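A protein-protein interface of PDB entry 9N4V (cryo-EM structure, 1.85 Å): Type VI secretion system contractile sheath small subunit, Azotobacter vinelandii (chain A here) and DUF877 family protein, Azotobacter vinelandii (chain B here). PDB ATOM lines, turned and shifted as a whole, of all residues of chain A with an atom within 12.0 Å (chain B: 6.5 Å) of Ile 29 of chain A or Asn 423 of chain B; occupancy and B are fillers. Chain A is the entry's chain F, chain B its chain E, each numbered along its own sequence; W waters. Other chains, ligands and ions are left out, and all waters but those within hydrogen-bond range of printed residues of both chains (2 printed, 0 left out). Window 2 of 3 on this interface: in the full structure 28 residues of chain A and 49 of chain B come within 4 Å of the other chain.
OD1 of Asp 427 of chain B is in salt-bridge range of NZ of Lys 31 of chain A, at 3.0 Å. The side-chain amino group (NZ) of Lys 31 of chain A sits at hydrogen-bond distance from the backbone carbonyl oxygen (O) of Trp 424 of chain B (2.9 Å).
Tyr 420 of chain B touches Ile 29 of chain A. Asn 423 of chain B touches Ile 29 of chain A (ND2 to CD1, 3.7 Å). Ile 29 of chain A touches Trp 424 of chain B (CD1 to CA, 3.9 Å).
Of the printed residues of chain B, Ile 29 of chain A touches Tyr 420, Asn 423 and Trp 424. Asn 423 of chain B touches one residue of chain A. Tyr 420 of chain B touches one residue of chain A. Asn 422 of chain B touches none of the printed residues of chain A. No residue of chain A comes within 4 Å of Ala 426 of chain B. Printed residues of chain A within 4 Å of Asp 427 of chain B: Lys 31 (3.0 Å). Printed residues of chain A within 4 Å of Trp 424 of chain B: Ile 29 (3.9 Å) and Lys 31 (2.9 Å). Of the printed residues of chain B, Lys 31 of chain A touches Trp 424 and Asp 427. The nearest residue of chain B that does not touch Ile 29 of chain A is Asp 427 of chain B (5.8 Å). The nearest printed residue of chain A that does not touch Trp 424 of chain B is Glu 30 of chain A (4.8 Å).
Of the 11 printed residues of chain A, 2 touch a printed residue of chain B. Of the 10 printed residues of chain B, 4 touch a printed residue of chain A. Printed residues of chain B that touch a printed residue of chain A: Tyr 420, Asn 423, Trp 424 and Asp 427. Hydrophobic or aromatic side chains of chain B that line the printed part of chain A: Tyr 420 and Trp 424. Among the printed residues, Asp or Glu carboxylates within 4 Å of a Lys or Arg side-chain nitrogen of the other chain: Lys 31 of chain A with Asp 427 of chain B.
Water W2 lies within hydrogen-bond range of ND2 of Asn 423 of chain B and O of Asn 27 of chain A. Water W1 bridges the backbone carbonyl oxygen (O) of Glu 30 of chain A (2.7 Å) and the side-chain hydroxyl (OH) of Tyr 420 of chain B (2.8 Å).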
ATOM      1  N   VAL A  23     -12.347 -18.823  -1.283  1.00  0.00           N
ATOM      2  CA  VAL A  23     -13.106 -17.684  -0.785  1.00  0.00           C
ATOM      3  C   VAL A  23     -13.610 -16.882  -1.977  1.00  0.00           C
ATOM      4  O   VAL A  23     -12.825 -16.465  -2.832  1.00  0.00           O
ATOM      5  CB  VAL A  23     -12.247 -16.809   0.142  1.00  0.00           C
ATOM      6  CG1 VAL A  23     -13.034 -15.592   0.594  1.00  0.00           C
ATOM      7  CG2 VAL A  23     -11.759 -17.617   1.330  1.00  0.00           C
ATOM      8  N   GLU A  24     -14.917 -16.665  -2.033  1.00  0.00           N
ATOM      9  CA  GLU A  24     -15.529 -15.902  -3.120  1.00  0.00           C
ATOM     10  C   GLU A  24     -15.363 -14.416  -2.822  1.00  0.00           C
ATOM     11  O   GLU A  24     -16.070 -13.859  -1.983  1.00  0.00           O
ATOM     12  CB  GLU A  24     -16.999 -16.274  -3.272  1.00  0.00           C
ATOM     13  CG  GLU A  24     -17.759 -15.403  -4.249  1.00  0.00           C
ATOM     14  CD  GLU A  24     -17.254 -15.548  -5.664  1.00  0.00           C
ATOM     15  OE1 GLU A  24     -16.953 -16.685  -6.075  1.00  0.00           O
ATOM     16  OE2 GLU A  24     -17.153 -14.525  -6.370  1.00  0.00           O
ATOM     17  N   THR A  25     -14.423 -13.767  -3.508  1.00  0.00           N
ATOM     18  CA  THR A  25     -14.151 -12.353  -3.287  1.00  0.00           C
ATOM     19  C   THR A  25     -14.548 -11.462  -4.454  1.00  0.00           C
ATOM     20  O   THR A  25     -14.475 -10.237  -4.320  1.00  0.00           O
ATOM     21  CB  THR A  25     -12.663 -12.132  -2.973  1.00  0.00           C
ATOM     22  OG1 THR A  25     -11.869 -12.481  -4.112  1.00  0.00           O
ATOM     23  CG2 THR A  25     -12.234 -12.970  -1.784  1.00  0.00           C
ATOM     24  N   GLY A  26     -14.962 -12.030  -5.582  1.00  0.00           N
ATOM     25  CA  GLY A  26     -15.361 -11.212  -6.716  1.00  0.00           C
ATOM     26  C   GLY A  26     -14.227 -10.314  -7.176  1.00  0.00           C
ATOM     27  O   GLY A  26     -13.076 -10.740  -7.301  1.00  0.00           O
ATOM     28  N   ASN A  27     -14.549  -9.044  -7.411  1.00  0.00           N
ATOM     29  CA  ASN A  27     -13.574  -8.050  -7.835  1.00  0.00           C
ATOM     30  C   ASN A  27     -13.042  -7.213  -6.674  1.00  0.00           C
ATOM     31  O   ASN A  27     -12.504  -6.127  -6.900  1.00  0.00           O
ATOM     32  CB  ASN A  27     -14.180  -7.138  -8.902  1.00  0.00           C
ATOM     33  CG  ASN A  27     -14.702  -7.906 -10.094  1.00  0.00           C
ATOM     34  OD1 ASN A  27     -14.110  -8.896 -10.518  1.00  0.00           O
ATOM     35  ND2 ASN A  27     -15.821  -7.451 -10.644  1.00  0.00           N
ATOM     36  N   ALA A  28     -13.185  -7.690  -5.442  1.00  0.00           N
ATOM     37  CA  ALA A  28     -12.749  -6.916  -4.290  1.00  0.00           C
ATOM     38  C   ALA A  28     -11.227  -6.853  -4.209  1.00  0.00           C
ATOM     39  O   ALA A  28     -10.521  -7.762  -4.647  1.00  0.00           O
ATOM     40  CB  ALA A  28     -13.308  -7.510  -2.999  1.00  0.00           C
ATOM     41  N   ILE A  29     -10.729  -5.765  -3.634  1.00  0.00           N
ATOM     42  CA  ILE A  29      -9.309  -5.581  -3.372  1.00  0.00           C
ATOM     43  C   ILE A  29      -9.086  -5.621  -1.869  1.00  0.00           C
ATOM     44  O   ILE A  29      -9.959  -5.243  -1.080  1.00  0.00           O
ATOM     45  CB  ILE A  29      -8.774  -4.261  -3.972  1.00  0.00           C
ATOM     46  CG1 ILE A  29      -9.521  -3.062  -3.379  1.00  0.00           C
ATOM     47  CG2 ILE A  29      -8.898  -4.279  -5.487  1.00  0.00           C
ATOM     48  CD1 ILE A  29      -8.994  -1.712  -3.833  1.00  0.00           C
ATOM     49  N   GLU A  30      -7.914  -6.101  -1.472  1.00  0.00           N
ATOM     50  CA  GLU A  30      -7.561  -6.150  -0.062  1.00  0.00           C
ATOM     51  C   GLU A  30      -7.289  -4.751   0.470  1.00  0.00           C
ATOM     52  O   GLU A  30      -6.671  -3.924  -0.202  1.00  0.00           O
ATOM     53  CB  GLU A  30      -6.338  -7.036   0.148  1.00  0.00           C
ATOM     54  CG  GLU A  30      -6.668  -8.492   0.372  1.00  0.00           C
ATOM     55  CD  GLU A  30      -5.434  -9.346   0.574  1.00  0.00           C
ATOM     56  OE1 GLU A  30      -4.906  -9.366   1.703  1.00  0.00           O
ATOM     57  OE2 GLU A  30      -4.999 -10.002  -0.396  1.00  0.00           O
ATOM     58  N   LYS A  31      -7.755  -4.486   1.685  1.00  0.00           N
ATOM     59  CA  LYS A  31      -7.594  -3.184   2.325  1.00  0.00           C
ATOM     60  C   LYS A  31      -6.675  -3.359   3.528  1.00  0.00           C
ATOM     61  O   LYS A  31      -7.123  -3.674   4.630  1.00  0.00           O
ATOM     62  CB  LYS A  31      -8.939  -2.600   2.734  1.00  0.00           C
ATOM     63  CG  LYS A  31      -9.863  -2.297   1.573  1.00  0.00           C
ATOM     64  CD  LYS A  31      -9.317  -1.175   0.706  1.00  0.00           C
ATOM     65  CE  LYS A  31      -9.207   0.125   1.487  1.00  0.00           C
ATOM     66  NZ  LYS A  31     -10.095   1.173   0.916  1.00  0.00           N
ATOM     67  N   LYS A  32      -5.380  -3.156   3.311  1.00  0.00           N
ATOM     68  CA  LYS A  32      -4.440  -3.176   4.420  1.00  0.00           C
ATOM     69  C   LYS A  32      -4.564  -1.894   5.233  1.00  0.00           C
ATOM     70  O   LYS A  32      -4.658  -0.796   4.681  1.00  0.00           O
ATOM     71  CB  LYS A  32      -3.011  -3.346   3.909  1.00  0.00           C
ATOM     72  CG  LYS A  32      -2.655  -4.768   3.508  1.00  0.00           C
ATOM     73  CD  LYS A  32      -1.229  -4.839   2.981  1.00  0.00           C
ATOM     74  CE  LYS A  32      -0.838  -6.257   2.614  1.00  0.00           C
ATOM     75  NZ  LYS A  32       0.553  -6.322   2.082  1.00  0.00           N
ATOM     76  N   GLU A  33      -4.577  -2.040   6.550  1.00  0.00           N
ATOM     77  CA  GLU A  33      -4.703  -0.912   7.459  1.00  0.00           C
ATOM     78  C   GLU A  33      -3.353  -0.594   8.086  1.00  0.00           C
ATOM     79  O   GLU A  33      -2.581  -1.498   8.412  1.00  0.00           O
ATOM     80  CB  GLU A  33      -5.730  -1.203   8.554  1.00  0.00           C
ATOM     81  CG  GLU A  33      -7.136  -1.452   8.036  1.00  0.00           C
ATOM     82  CD  GLU A  33      -7.761  -0.215   7.423  1.00  0.00           C
ATOM     83  OE1 GLU A  33      -7.539   0.034   6.218  1.00  0.00           O
ATOM     84  OE2 GLU A  33      -8.474   0.510   8.149  1.00  0.00           O
ATOM     85  N   GLN B 418      -4.587   3.719 -12.396  1.00  0.00           N
ATOM     86  CA  GLN B 418      -5.616   4.714 -12.113  1.00  0.00           C
ATOM     87  C   GLN B 418      -6.868   4.066 -11.530  1.00  0.00           C
ATOM     88  O   GLN B 418      -7.425   4.545 -10.535  1.00  0.00           O
ATOM     89  CB  GLN B 418      -5.952   5.487 -13.385  1.00  0.00           C
ATOM     90  CG  GLN B 418      -6.875   6.665 -13.158  1.00  0.00           C
ATOM     91  CD  GLN B 418      -6.924   7.583 -14.355  1.00  0.00           C
ATOM     92  OE1 GLN B 418      -5.983   8.322 -14.621  1.00  0.00           O
ATOM     93  NE2 GLN B 418      -8.026   7.533 -15.090  1.00  0.00           N
ATOM     94  N   THR B 419      -7.315   2.966 -12.136  1.00  0.00           N
ATOM     95  CA  THR B 419      -8.492   2.266 -11.638  1.00  0.00           C
ATOM     96  C   THR B 419      -8.269   1.766 -10.220  1.00  0.00           C
ATOM     97  O   THR B 419      -9.136   1.928  -9.358  1.00  0.00           O
ATOM     98  CB  THR B 419      -8.845   1.102 -12.565  1.00  0.00           C
ATOM     99  OG1 THR B 419      -9.343   1.615 -13.805  1.00  0.00           O
ATOM    100  CG2 THR B 419      -9.900   0.211 -11.935  1.00  0.00           C
ATOM    101  N   TYR B 420      -7.107   1.166  -9.954  1.00  0.00           N
ATOM    102  CA  TYR B 420      -6.839   0.652  -8.618  1.00  0.00           C
ATOM    103  C   TYR B 420      -6.855   1.773  -7.586  1.00  0.00           C
ATOM    104  O   TYR B 420      -7.498   1.654  -6.540  1.00  0.00           O
ATOM    105  CB  TYR B 420      -5.500  -0.082  -8.591  1.00  0.00           C
ATOM    106  CG  TYR B 420      -5.092  -0.512  -7.206  1.00  0.00           C
ATOM    107  CD1 TYR B 420      -5.742  -1.556  -6.566  1.00  0.00           C
ATOM    108  CD2 TYR B 420      -4.069   0.134  -6.529  1.00  0.00           C
ATOM    109  CE1 TYR B 420      -5.382  -1.949  -5.298  1.00  0.00           C
ATOM    110  CE2 TYR B 420      -3.699  -0.256  -5.260  1.00  0.00           C
ATOM    111  CZ  TYR B 420      -4.362  -1.299  -4.649  1.00  0.00           C
ATOM    112  OH  TYR B 420      -4.003  -1.697  -3.386  1.00  0.00           O
ATOM    113  N   LEU B 421      -6.165   2.878  -7.871  1.00  0.00           N
ATOM    114  CA  LEU B 421      -6.068   3.947  -6.883  1.00  0.00           C
ATOM    115  C   LEU B 421      -7.416   4.624  -6.649  1.00  0.00           C
ATOM    116  O   LEU B 421      -7.752   4.962  -5.511  1.00  0.00           O
ATOM    117  CB  LEU B 421      -5.010   4.959  -7.309  1.00  0.00           C
ATOM    118  CG  LEU B 421      -3.575   4.452  -7.159  1.00  0.00           C
ATOM    119  CD1 LEU B 421      -2.579   5.536  -7.521  1.00  0.00           C
ATOM    120  CD2 LEU B 421      -3.341   3.940  -5.745  1.00  0.00           C
ATOM    121  N   ASN B 422      -8.205   4.828  -7.707  1.00  0.00           N
ATOM    122  CA  ASN B 422      -9.524   5.423  -7.513  1.00  0.00           C
ATOM    123  C   ASN B 422     -10.471   4.471  -6.795  1.00  0.00           C
ATOM    124  O   ASN B 422     -11.317   4.918  -6.014  1.00  0.00           O
ATOM    125  CB  ASN B 422     -10.114   5.854  -8.852  1.00  0.00           C
ATOM    126  CG  ASN B 422      -9.581   7.194  -9.309  1.00  0.00           C
ATOM    127  OD1 ASN B 422      -9.867   8.223  -8.704  1.00  0.00           O
ATOM    128  ND2 ASN B 422      -8.798   7.188 -10.377  1.00  0.00           N
ATOM    129  N   ASN B 423     -10.357   3.166  -7.050  1.00  0.00           N
ATOM    130  CA  ASN B 423     -11.158   2.195  -6.314  1.00  0.00           C
ATOM    131  C   ASN B 423     -10.791   2.189  -4.838  1.00  0.00           C
ATOM    132  O   ASN B 423     -11.671   2.166  -3.973  1.00  0.00           O
ATOM    133  CB  ASN B 423     -10.966   0.805  -6.920  1.00  0.00           C
ATOM    134  CG  ASN B 423     -11.913  -0.222  -6.341  1.00  0.00           C
ATOM    135  OD1 ASN B 423     -12.939   0.116  -5.756  1.00  0.00           O
ATOM    136  ND2 ASN B 423     -11.570  -1.493  -6.502  1.00  0.00           N
ATOM    137  N   TRP B 424      -9.494   2.223  -4.537  1.00  0.00           N
ATOM    138  CA  TRP B 424      -9.040   2.129  -3.154  1.00  0.00           C
ATOM    139  C   TRP B 424      -9.473   3.342  -2.336  1.00  0.00           C
ATOM    140  O   TRP B 424      -9.901   3.198  -1.188  1.00  0.00           O
ATOM    141  CB  TRP B 424      -7.520   1.964  -3.119  1.00  0.00           C
ATOM    142  CG  TRP B 424      -6.957   1.949  -1.740  1.00  0.00           C
ATOM    143  CD1 TRP B 424      -6.736   0.858  -0.956  1.00  0.00           C
ATOM    144  CD2 TRP B 424      -6.547   3.084  -0.975  1.00  0.00           C
ATOM    145  NE1 TRP B 424      -6.212   1.244   0.252  1.00  0.00           N
ATOM    146  CE2 TRP B 424      -6.088   2.607   0.265  1.00  0.00           C
ATOM    147  CE3 TRP B 424      -6.522   4.458  -1.220  1.00  0.00           C
ATOM    148  CZ2 TRP B 424      -5.612   3.456   1.259  1.00  0.00           C
ATOM    149  CZ3 TRP B 424      -6.048   5.299  -0.232  1.00  0.00           C
ATOM    150  CH2 TRP B 424      -5.600   4.794   0.991  1.00  0.00           C
ATOM    151  N   ILE B 425      -9.376   4.543  -2.911  1.00  0.00           N
ATOM    152  CA  ILE B 425      -9.675   5.763  -2.161  1.00  0.00           C
ATOM    153  C   ILE B 425     -11.165   6.009  -1.984  1.00  0.00           C
ATOM    154  O   ILE B 425     -11.550   6.813  -1.129  1.00  0.00           O
ATOM    155  CB  ILE B 425      -9.036   6.989  -2.841  1.00  0.00           C
ATOM    156  CG1 ILE B 425      -8.828   8.116  -1.828  1.00  0.00           C
ATOM    157  CG2 ILE B 425      -9.886   7.463  -4.005  1.00  0.00           C
ATOM    158  CD1 ILE B 425      -7.848   9.154  -2.279  1.00  0.00           C
ATOM    159  N   ALA B 426     -12.014   5.320  -2.748  1.00  0.00           N
ATOM    160  CA  ALA B 426     -13.447   5.583  -2.691  1.00  0.00           C
ATOM    161  C   ALA B 426     -14.043   5.253  -1.326  1.00  0.00           C
ATOM    162  O   ALA B 426     -15.076   5.815  -0.954  1.00  0.00           O
ATOM    163  CB  ALA B 426     -14.167   4.792  -3.779  1.00  0.00           C
ATOM    164  N   ASP B 427     -13.421   4.344  -0.575  1.00  0.00           N
ATOM    165  CA  ASP B 427     -13.965   3.950   0.719  1.00  0.00           C
ATOM    166  C   ASP B 427     -13.882   5.059   1.763  1.00  0.00           C
ATOM    167  O   ASP B 427     -14.568   4.980   2.786  1.00  0.00           O
ATOM    168  CB  ASP B 427     -13.241   2.708   1.236  1.00  0.00           C
ATOM    169  CG  ASP B 427     -13.315   1.547   0.265  1.00  0.00           C
ATOM    170  OD1 ASP B 427     -12.602   1.576  -0.763  1.00  0.00           O
ATOM    171  OD2 ASP B 427     -14.083   0.601   0.538  1.00  0.00           O
HETATM  172  O   HOH W   1      -5.139  -4.074  -2.448  1.00  0.00           O
HETATM  173  O   HOH W   2     -13.126  -3.453  -5.895  1.00  0.00           O
